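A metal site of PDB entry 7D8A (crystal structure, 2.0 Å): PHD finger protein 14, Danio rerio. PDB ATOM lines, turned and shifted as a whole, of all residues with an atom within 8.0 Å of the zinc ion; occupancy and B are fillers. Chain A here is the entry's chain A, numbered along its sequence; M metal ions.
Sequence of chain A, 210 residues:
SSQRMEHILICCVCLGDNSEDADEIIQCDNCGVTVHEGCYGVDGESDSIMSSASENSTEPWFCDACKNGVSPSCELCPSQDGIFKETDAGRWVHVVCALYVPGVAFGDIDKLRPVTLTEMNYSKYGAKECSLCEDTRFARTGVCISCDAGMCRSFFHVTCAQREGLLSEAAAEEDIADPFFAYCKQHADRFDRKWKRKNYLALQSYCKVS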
ATOM      1  N   SER A  73      29.112 -26.731  -6.456  1.00  0.00           N
ATOM      2  CA  SER A  73      27.887 -27.452  -6.745  1.00  0.00           C
ATOM      3  C   SER A  73      27.640 -28.468  -5.640  1.00  0.00           C
ATOM      4  O   SER A  73      28.525 -28.790  -4.845  1.00  0.00           O
ATOM      5  CB  SER A  73      27.949 -28.129  -8.114  1.00  0.00           C
ATOM      6  OG  SER A  73      29.039 -29.004  -8.176  1.00  0.00           O
ATOM      7  N   CYS A  74      26.412 -28.956  -5.583  1.00  0.00           N
ATOM      8  CA  CYS A  74      25.989 -29.874  -4.545  1.00  0.00           C
ATOM      9  C   CYS A  74      26.088 -31.311  -5.047  1.00  0.00           C
ATOM     10  O   CYS A  74      25.766 -31.598  -6.204  1.00  0.00           O
ATOM     11  CB  CYS A  74      24.550 -29.550  -4.114  1.00  0.00           C
ATOM     12  SG  CYS A  74      23.902 -30.619  -2.833  1.00  0.00           S
ATOM     13  N   GLU A  75      26.583 -32.200  -4.181  1.00  0.00           N
ATOM     14  CA  GLU A  75      26.625 -33.628  -4.518  1.00  0.00           C
ATOM     15  C   GLU A  75      25.231 -34.236  -4.642  1.00  0.00           C
ATOM     16  O   GLU A  75      25.101 -35.316  -5.222  1.00  0.00           O
ATOM     17  CB  GLU A  75      27.413 -34.387  -3.446  1.00  0.00           C
ATOM     18  CG  GLU A  75      28.891 -34.049  -3.377  1.00  0.00           C
ATOM     19  CD  GLU A  75      29.623 -34.474  -4.615  1.00  0.00           C
ATOM     20  OE1 GLU A  75      30.007 -35.658  -4.714  1.00  0.00           O
ATOM     21  OE2 GLU A  75      29.812 -33.629  -5.503  1.00  0.00           O
ATOM     22  N   LEU A  76      24.199 -33.572  -4.128  1.00  0.00           N
ATOM     23  CA  LEU A  76      22.874 -34.172  -3.989  1.00  0.00           C
ATOM     24  C   LEU A  76      21.791 -33.515  -4.845  1.00  0.00           C
ATOM     25  O   LEU A  76      20.647 -33.976  -4.800  1.00  0.00           O
ATOM     26  CB  LEU A  76      22.437 -34.133  -2.507  1.00  0.00           C
ATOM     27  CG  LEU A  76      23.349 -34.860  -1.503  1.00  0.00           C
ATOM     28  CD1 LEU A  76      22.839 -34.709  -0.066  1.00  0.00           C
ATOM     29  CD2 LEU A  76      23.480 -36.327  -1.854  1.00  0.00           C
ATOM     30  N   CYS A  77      22.122 -32.512  -5.652  1.00  0.00           N
ATOM     31  CA  CYS A  77      21.109 -31.829  -6.461  1.00  0.00           C
ATOM     32  C   CYS A  77      21.797 -30.915  -7.472  1.00  0.00           C
ATOM     33  O   CYS A  77      22.998 -30.672  -7.348  1.00  0.00           O
ATOM     34  CB  CYS A  77      20.152 -31.023  -5.568  1.00  0.00           C
ATOM     35  SG  CYS A  77      20.781 -29.402  -5.020  1.00  0.00           S
ATOM     36  N   PRO A  78      21.089 -30.394  -8.482  1.00  0.00           N
ATOM     37  CA  PRO A  78      21.757 -29.564  -9.495  1.00  0.00           C
ATOM     38  C   PRO A  78      21.734 -28.066  -9.246  1.00  0.00           C
ATOM     39  O   PRO A  78      22.189 -27.313 -10.115  1.00  0.00           O
ATOM     40  CB  PRO A  78      20.948 -29.888 -10.756  1.00  0.00           C
ATOM     41  CG  PRO A  78      19.539 -30.072 -10.224  1.00  0.00           C
ATOM     42  CD  PRO A  78      19.711 -30.728  -8.863  1.00  0.00           C
ATOM     43  N   SER A  79      21.213 -27.586  -8.108  1.00  0.00           N
ATOM     44  CA  SER A  79      21.124 -26.153  -7.879  1.00  0.00           C
ATOM     45  C   SER A  79      22.448 -25.570  -7.416  1.00  0.00           C
ATOM     46  O   SER A  79      23.200 -26.203  -6.670  1.00  0.00           O
ATOM     47  CB  SER A  79      20.069 -25.823  -6.826  1.00  0.00           C
ATOM     48  OG  SER A  79      20.189 -24.472  -6.405  1.00  0.00           O
ATOM     49  N   GLN A  80      22.691 -24.307  -7.801  1.00  0.00           N
ATOM     50  CA  GLN A  80      23.897 -23.557  -7.447  1.00  0.00           C
ATOM     51  C   GLN A  80      23.656 -22.481  -6.409  1.00  0.00           C
ATOM     52  O   GLN A  80      24.615 -21.823  -5.965  1.00  0.00           O
ATOM     53  CB  GLN A  80      24.491 -22.890  -8.693  1.00  0.00           C
ATOM     54  CG  GLN A  80      24.661 -23.797  -9.885  1.00  0.00           C
ATOM     55  CD  GLN A  80      25.860 -24.682  -9.747  1.00  0.00           C
ATOM     56  OE1 GLN A  80      25.746 -25.915  -9.724  1.00  0.00           O
ATOM     57  NE2 GLN A  80      27.038 -24.068  -9.634  1.00  0.00           N
ATOM     58  N   ASP A  81      22.399 -22.239  -6.044  1.00  0.00           N
ATOM     59  CA  ASP A  81      22.038 -21.203  -5.088  1.00  0.00           C
ATOM     60  C   ASP A  81      21.970 -21.797  -3.687  1.00  0.00           C
ATOM     61  O   ASP A  81      22.093 -23.008  -3.492  1.00  0.00           O
ATOM     62  CB  ASP A  81      20.695 -20.579  -5.457  1.00  0.00           C
ATOM     63  CG  ASP A  81      20.453 -20.528  -6.952  1.00  0.00           C
ATOM     64  OD1 ASP A  81      21.377 -20.128  -7.691  1.00  0.00           O
ATOM     65  OD2 ASP A  81      19.342 -20.906  -7.392  1.00  0.00           O
ATOM     66  N   ILE A  83      23.017 -22.226   0.462  1.00  0.00           N
ATOM     67  CA  ILE A  83      24.210 -22.237   1.300  1.00  0.00           C
ATOM     68  C   ILE A  83      24.679 -23.681   1.502  1.00  0.00           C
ATOM     69  O   ILE A  83      23.848 -24.610   1.569  1.00  0.00           O
ATOM     70  CB  ILE A  83      23.939 -21.499   2.633  1.00  0.00           C
ATOM     71  CG1 ILE A  83      25.259 -21.030   3.253  1.00  0.00           C
ATOM     72  CG2 ILE A  83      23.061 -22.318   3.565  1.00  0.00           C
ATOM     73  CD1 ILE A  83      25.070 -20.146   4.455  1.00  0.00           C
ATOM     74  N   PHE A  84      25.999 -23.857   1.554  1.00  0.00           N
ATOM     75  CA  PHE A  84      26.658 -25.164   1.449  1.00  0.00           C
ATOM     76  C   PHE A  84      27.521 -25.468   2.666  1.00  0.00           C
ATOM     77  O   PHE A  84      27.984 -24.560   3.376  1.00  0.00           O
ATOM     78  CB  PHE A  84      27.571 -25.226   0.209  1.00  0.00           C
ATOM     79  CG  PHE A  84      26.846 -25.145  -1.102  1.00  0.00           C
ATOM     80  CD1 PHE A  84      26.548 -26.294  -1.808  1.00  0.00           C
ATOM     81  CD2 PHE A  84      26.460 -23.918  -1.621  1.00  0.00           C
ATOM     82  CE1 PHE A  84      25.881 -26.226  -3.029  1.00  0.00           C
ATOM     83  CE2 PHE A  84      25.791 -23.837  -2.843  1.00  0.00           C
ATOM     84  CZ  PHE A  84      25.509 -24.996  -3.546  1.00  0.00           C
ATOM     85  N   TRP A  92      30.914 -30.779  -1.620  1.00  0.00           N
ATOM     86  CA  TRP A  92      29.979 -29.814  -1.040  1.00  0.00           C
ATOM     87  C   TRP A  92      28.540 -30.280  -1.188  1.00  0.00           C
ATOM     88  O   TRP A  92      28.175 -30.912  -2.184  1.00  0.00           O
ATOM     89  CB  TRP A  92      30.149 -28.421  -1.686  1.00  0.00           C
ATOM     90  CG  TRP A  92      31.528 -27.885  -1.494  1.00  0.00           C
ATOM     91  CD1 TRP A  92      32.630 -28.141  -2.255  1.00  0.00           C
ATOM     92  CD2 TRP A  92      31.975 -27.028  -0.434  1.00  0.00           C
ATOM     93  NE1 TRP A  92      33.728 -27.494  -1.750  1.00  0.00           N
ATOM     94  CE2 TRP A  92      33.351 -26.798  -0.631  1.00  0.00           C
ATOM     95  CE3 TRP A  92      31.342 -26.420   0.661  1.00  0.00           C
ATOM     96  CZ2 TRP A  92      34.108 -25.995   0.214  1.00  0.00           C
ATOM     97  CZ3 TRP A  92      32.086 -25.621   1.495  1.00  0.00           C
ATOM     98  CH2 TRP A  92      33.462 -25.416   1.281  1.00  0.00           C
ATOM     99  N   VAL A  93      27.735 -29.946  -0.182  1.00  0.00           N
ATOM    100  CA  VAL A  93      26.313 -30.248  -0.167  1.00  0.00           C
ATOM    101  C   VAL A  93      25.568 -29.049   0.409  1.00  0.00           C
ATOM    102  O   VAL A  93      26.079 -28.342   1.274  1.00  0.00           O
ATOM    103  CB  VAL A  93      25.973 -31.527   0.645  1.00  0.00           C
ATOM    104  CG1 VAL A  93      26.645 -32.735   0.030  1.00  0.00           C
ATOM    105  CG2 VAL A  93      26.377 -31.363   2.094  1.00  0.00           C
ATOM    106  N   HIS A  94      24.355 -28.816  -0.094  1.00  0.00           N
ATOM    107  CA  HIS A  94      23.490 -27.849   0.567  1.00  0.00           C
ATOM    108  C   HIS A  94      23.213 -28.331   1.976  1.00  0.00           C
ATOM    109  O   HIS A  94      23.034 -29.534   2.209  1.00  0.00           O
ATOM    110  CB  HIS A  94      22.145 -27.676  -0.140  1.00  0.00           C
ATOM    111  CG  HIS A  94      22.209 -26.990  -1.462  1.00  0.00           C
ATOM    112  ND1 HIS A  94      22.123 -27.679  -2.657  1.00  0.00           N
ATOM    113  CD2 HIS A  94      22.267 -25.667  -1.779  1.00  0.00           C
ATOM    114  CE1 HIS A  94      22.181 -26.807  -3.648  1.00  0.00           C
ATOM    115  NE2 HIS A  94      22.266 -25.587  -3.153  1.00  0.00           N
ATOM    116  N   VAL A  95      23.111 -27.394   2.908  1.00  0.00           N
ATOM    117  CA  VAL A  95      22.573 -27.731   4.221  1.00  0.00           C
ATOM    118  C   VAL A  95      21.197 -28.389   4.076  1.00  0.00           C
ATOM    119  O   VAL A  95      20.925 -29.429   4.673  1.00  0.00           O
ATOM    120  CB  VAL A  95      22.514 -26.482   5.109  1.00  0.00           C
ATOM    121  CG1 VAL A  95      21.739 -26.774   6.394  1.00  0.00           C
ATOM    122  CG2 VAL A  95      23.947 -26.017   5.440  1.00  0.00           C
ATOM    123  N   VAL A  96      20.314 -27.787   3.265  1.00  0.00           N
ATOM    124  CA  VAL A  96      18.950 -28.292   3.214  1.00  0.00           C
ATOM    125  C   VAL A  96      18.904 -29.691   2.596  1.00  0.00           C
ATOM    126  O   VAL A  96      18.150 -30.564   3.043  1.00  0.00           O
ATOM    127  CB  VAL A  96      18.019 -27.285   2.496  1.00  0.00           C
ATOM    128  CG1 VAL A  96      18.343 -27.133   1.015  1.00  0.00           C
ATOM    129  CG2 VAL A  96      16.555 -27.662   2.679  1.00  0.00           C
ATOM    130  N   CYS A  97      19.767 -29.956   1.599  1.00  0.00           N
ATOM    131  CA  CYS A  97      19.830 -31.319   1.052  1.00  0.00           C
ATOM    132  C   CYS A  97      20.271 -32.311   2.107  1.00  0.00           C
ATOM    133  O   CYS A  97      19.696 -33.408   2.221  1.00  0.00           O
ATOM    134  CB  CYS A  97      20.752 -31.375  -0.157  1.00  0.00           C
ATOM    135  SG  CYS A  97      20.047 -30.651  -1.641  1.00  0.00           S
ATOM    136  N   ALA A  98      21.280 -31.960   2.903  1.00  0.00           N
ATOM    137  CA  ALA A  98      21.772 -32.890   3.927  1.00  0.00           C
ATOM    138  C   ALA A  98      20.707 -33.155   4.985  1.00  0.00           C
ATOM    139  O   ALA A  98      20.599 -34.278   5.482  1.00  0.00           O
ATOM    140  CB  ALA A  98      23.026 -32.325   4.586  1.00  0.00           C
ATOM    141  N   VAL A 101      17.697 -35.424   2.961  1.00  0.00           N
ATOM    142  CA  VAL A 101      17.995 -36.701   2.303  1.00  0.00           C
ATOM    143  C   VAL A 101      18.268 -37.769   3.365  1.00  0.00           C
ATOM    144  O   VAL A 101      19.099 -37.533   4.263  1.00  0.00           O
ATOM    145  CB  VAL A 101      19.164 -36.556   1.336  1.00  0.00           C
ATOM    146  CG1 VAL A 101      19.679 -37.942   0.916  1.00  0.00           C
ATOM    147  CG2 VAL A 101      18.727 -35.745   0.091  1.00  0.00           C
ATOM    148  N   GLY A 142      22.134 -36.138  -9.016  1.00  0.00           N
ATOM    149  CA  GLY A 142      21.875 -36.007  -7.593  1.00  0.00           C
ATOM    150  C   GLY A 142      20.947 -37.072  -7.033  1.00  0.00           C
ATOM    151  O   GLY A 142      20.788 -38.167  -7.584  1.00  0.00           O
ATOM    152  N   VAL A 143      20.301 -36.724  -5.915  1.00  0.00           N
ATOM    153  CA  VAL A 143      19.484 -37.653  -5.154  1.00  0.00           C
ATOM    154  C   VAL A 143      18.120 -36.994  -4.889  1.00  0.00           C
ATOM    155  O   VAL A 143      18.069 -35.873  -4.370  1.00  0.00           O
ATOM    156  CB  VAL A 143      20.182 -38.070  -3.833  1.00  0.00           C
ATOM    157  CG1 VAL A 143      19.286 -38.964  -2.945  1.00  0.00           C
ATOM    158  CG2 VAL A 143      21.506 -38.801  -4.146  1.00  0.00           C
ATOM    159  N   HIS A 157      14.206 -33.467  -6.183  1.00  0.00           N
ATOM    160  CA  HIS A 157      15.352 -32.885  -5.490  1.00  0.00           C
ATOM    161  C   HIS A 157      14.888 -32.074  -4.285  1.00  0.00           C
ATOM    162  O   HIS A 157      13.814 -31.471  -4.319  1.00  0.00           O
ATOM    163  CB  HIS A 157      16.144 -31.980  -6.435  1.00  0.00           C
ATOM    164  CG  HIS A 157      16.851 -32.727  -7.522  1.00  0.00           C
ATOM    165  ND1 HIS A 157      16.629 -32.488  -8.856  1.00  0.00           N
ATOM    166  CD2 HIS A 157      17.795 -33.703  -7.469  1.00  0.00           C
ATOM    167  CE1 HIS A 157      17.383 -33.281  -9.586  1.00  0.00           C
ATOM    168  NE2 HIS A 157      18.111 -34.030  -8.767  1.00  0.00           N
ATOM    169  N   VAL A 158      15.689 -32.058  -3.230  1.00  0.00           N
ATOM    170  CA  VAL A 158      15.318 -31.278  -2.039  1.00  0.00           C
ATOM    171  C   VAL A 158      15.154 -29.810  -2.406  1.00  0.00           C
ATOM    172  O   VAL A 158      14.187 -29.147  -2.015  1.00  0.00           O
ATOM    173  CB  VAL A 158      16.344 -31.468  -0.916  1.00  0.00           C
ATOM    174  CG1 VAL A 158      16.019 -30.536   0.271  1.00  0.00           C
ATOM    175  CG2 VAL A 158      16.409 -32.923  -0.453  1.00  0.00           C
ATOM    176  N   THR A 159      16.118 -29.268  -3.157  1.00  0.00           N
ATOM    177  CA  THR A 159      16.055 -27.847  -3.514  1.00  0.00           C
ATOM    178  C   THR A 159      14.971 -27.551  -4.547  1.00  0.00           C
ATOM    179  O   THR A 159      14.476 -26.415  -4.600  1.00  0.00           O
ATOM    180  CB  THR A 159      17.429 -27.379  -3.995  1.00  0.00           C
ATOM    181  OG1 THR A 159      17.923 -28.313  -4.946  1.00  0.00           O
ATOM    182  CG2 THR A 159      18.452 -27.308  -2.815  1.00  0.00           C
ATOM    183  N   CYS A 160      14.583 -28.529  -5.369  1.00  0.00           N
ATOM    184  CA  CYS A 160      13.438 -28.308  -6.258  1.00  0.00           C
ATOM    185  C   CYS A 160      12.123 -28.293  -5.474  1.00  0.00           C
ATOM    186  O   CYS A 160      11.243 -27.480  -5.763  1.00  0.00           O
ATOM    187  CB  CYS A 160      13.386 -29.362  -7.370  1.00  0.00           C
ATOM    188  SG  CYS A 160      14.766 -29.239  -8.559  1.00  0.00           S
HETATM  189 ZN    ZN M   1      21.669 -29.698  -2.966  1.00  0.00          ZN
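The zinc ion is bound by ND1 of His 94 (2.1 Å), SG of Cys 77 (2.3 Å), SG of Cys 97 (2.3 Å) and SG of Cys 74 (2.4 Å).
The zinc ion has four donor atoms within binding distance.
NE2 of His 94 is in hydrogen-bond range of O of Asp 81.
The side-chain sulfur (SG) of Cys 77 lies close to the side-chain hydroxyl (OG1) of Thr 159 (3.1 Å).
SG of Cys 77 lies close to N of Ser 79 (3.6 Å).
SG of Cys 74 sits close to N of Leu 76.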
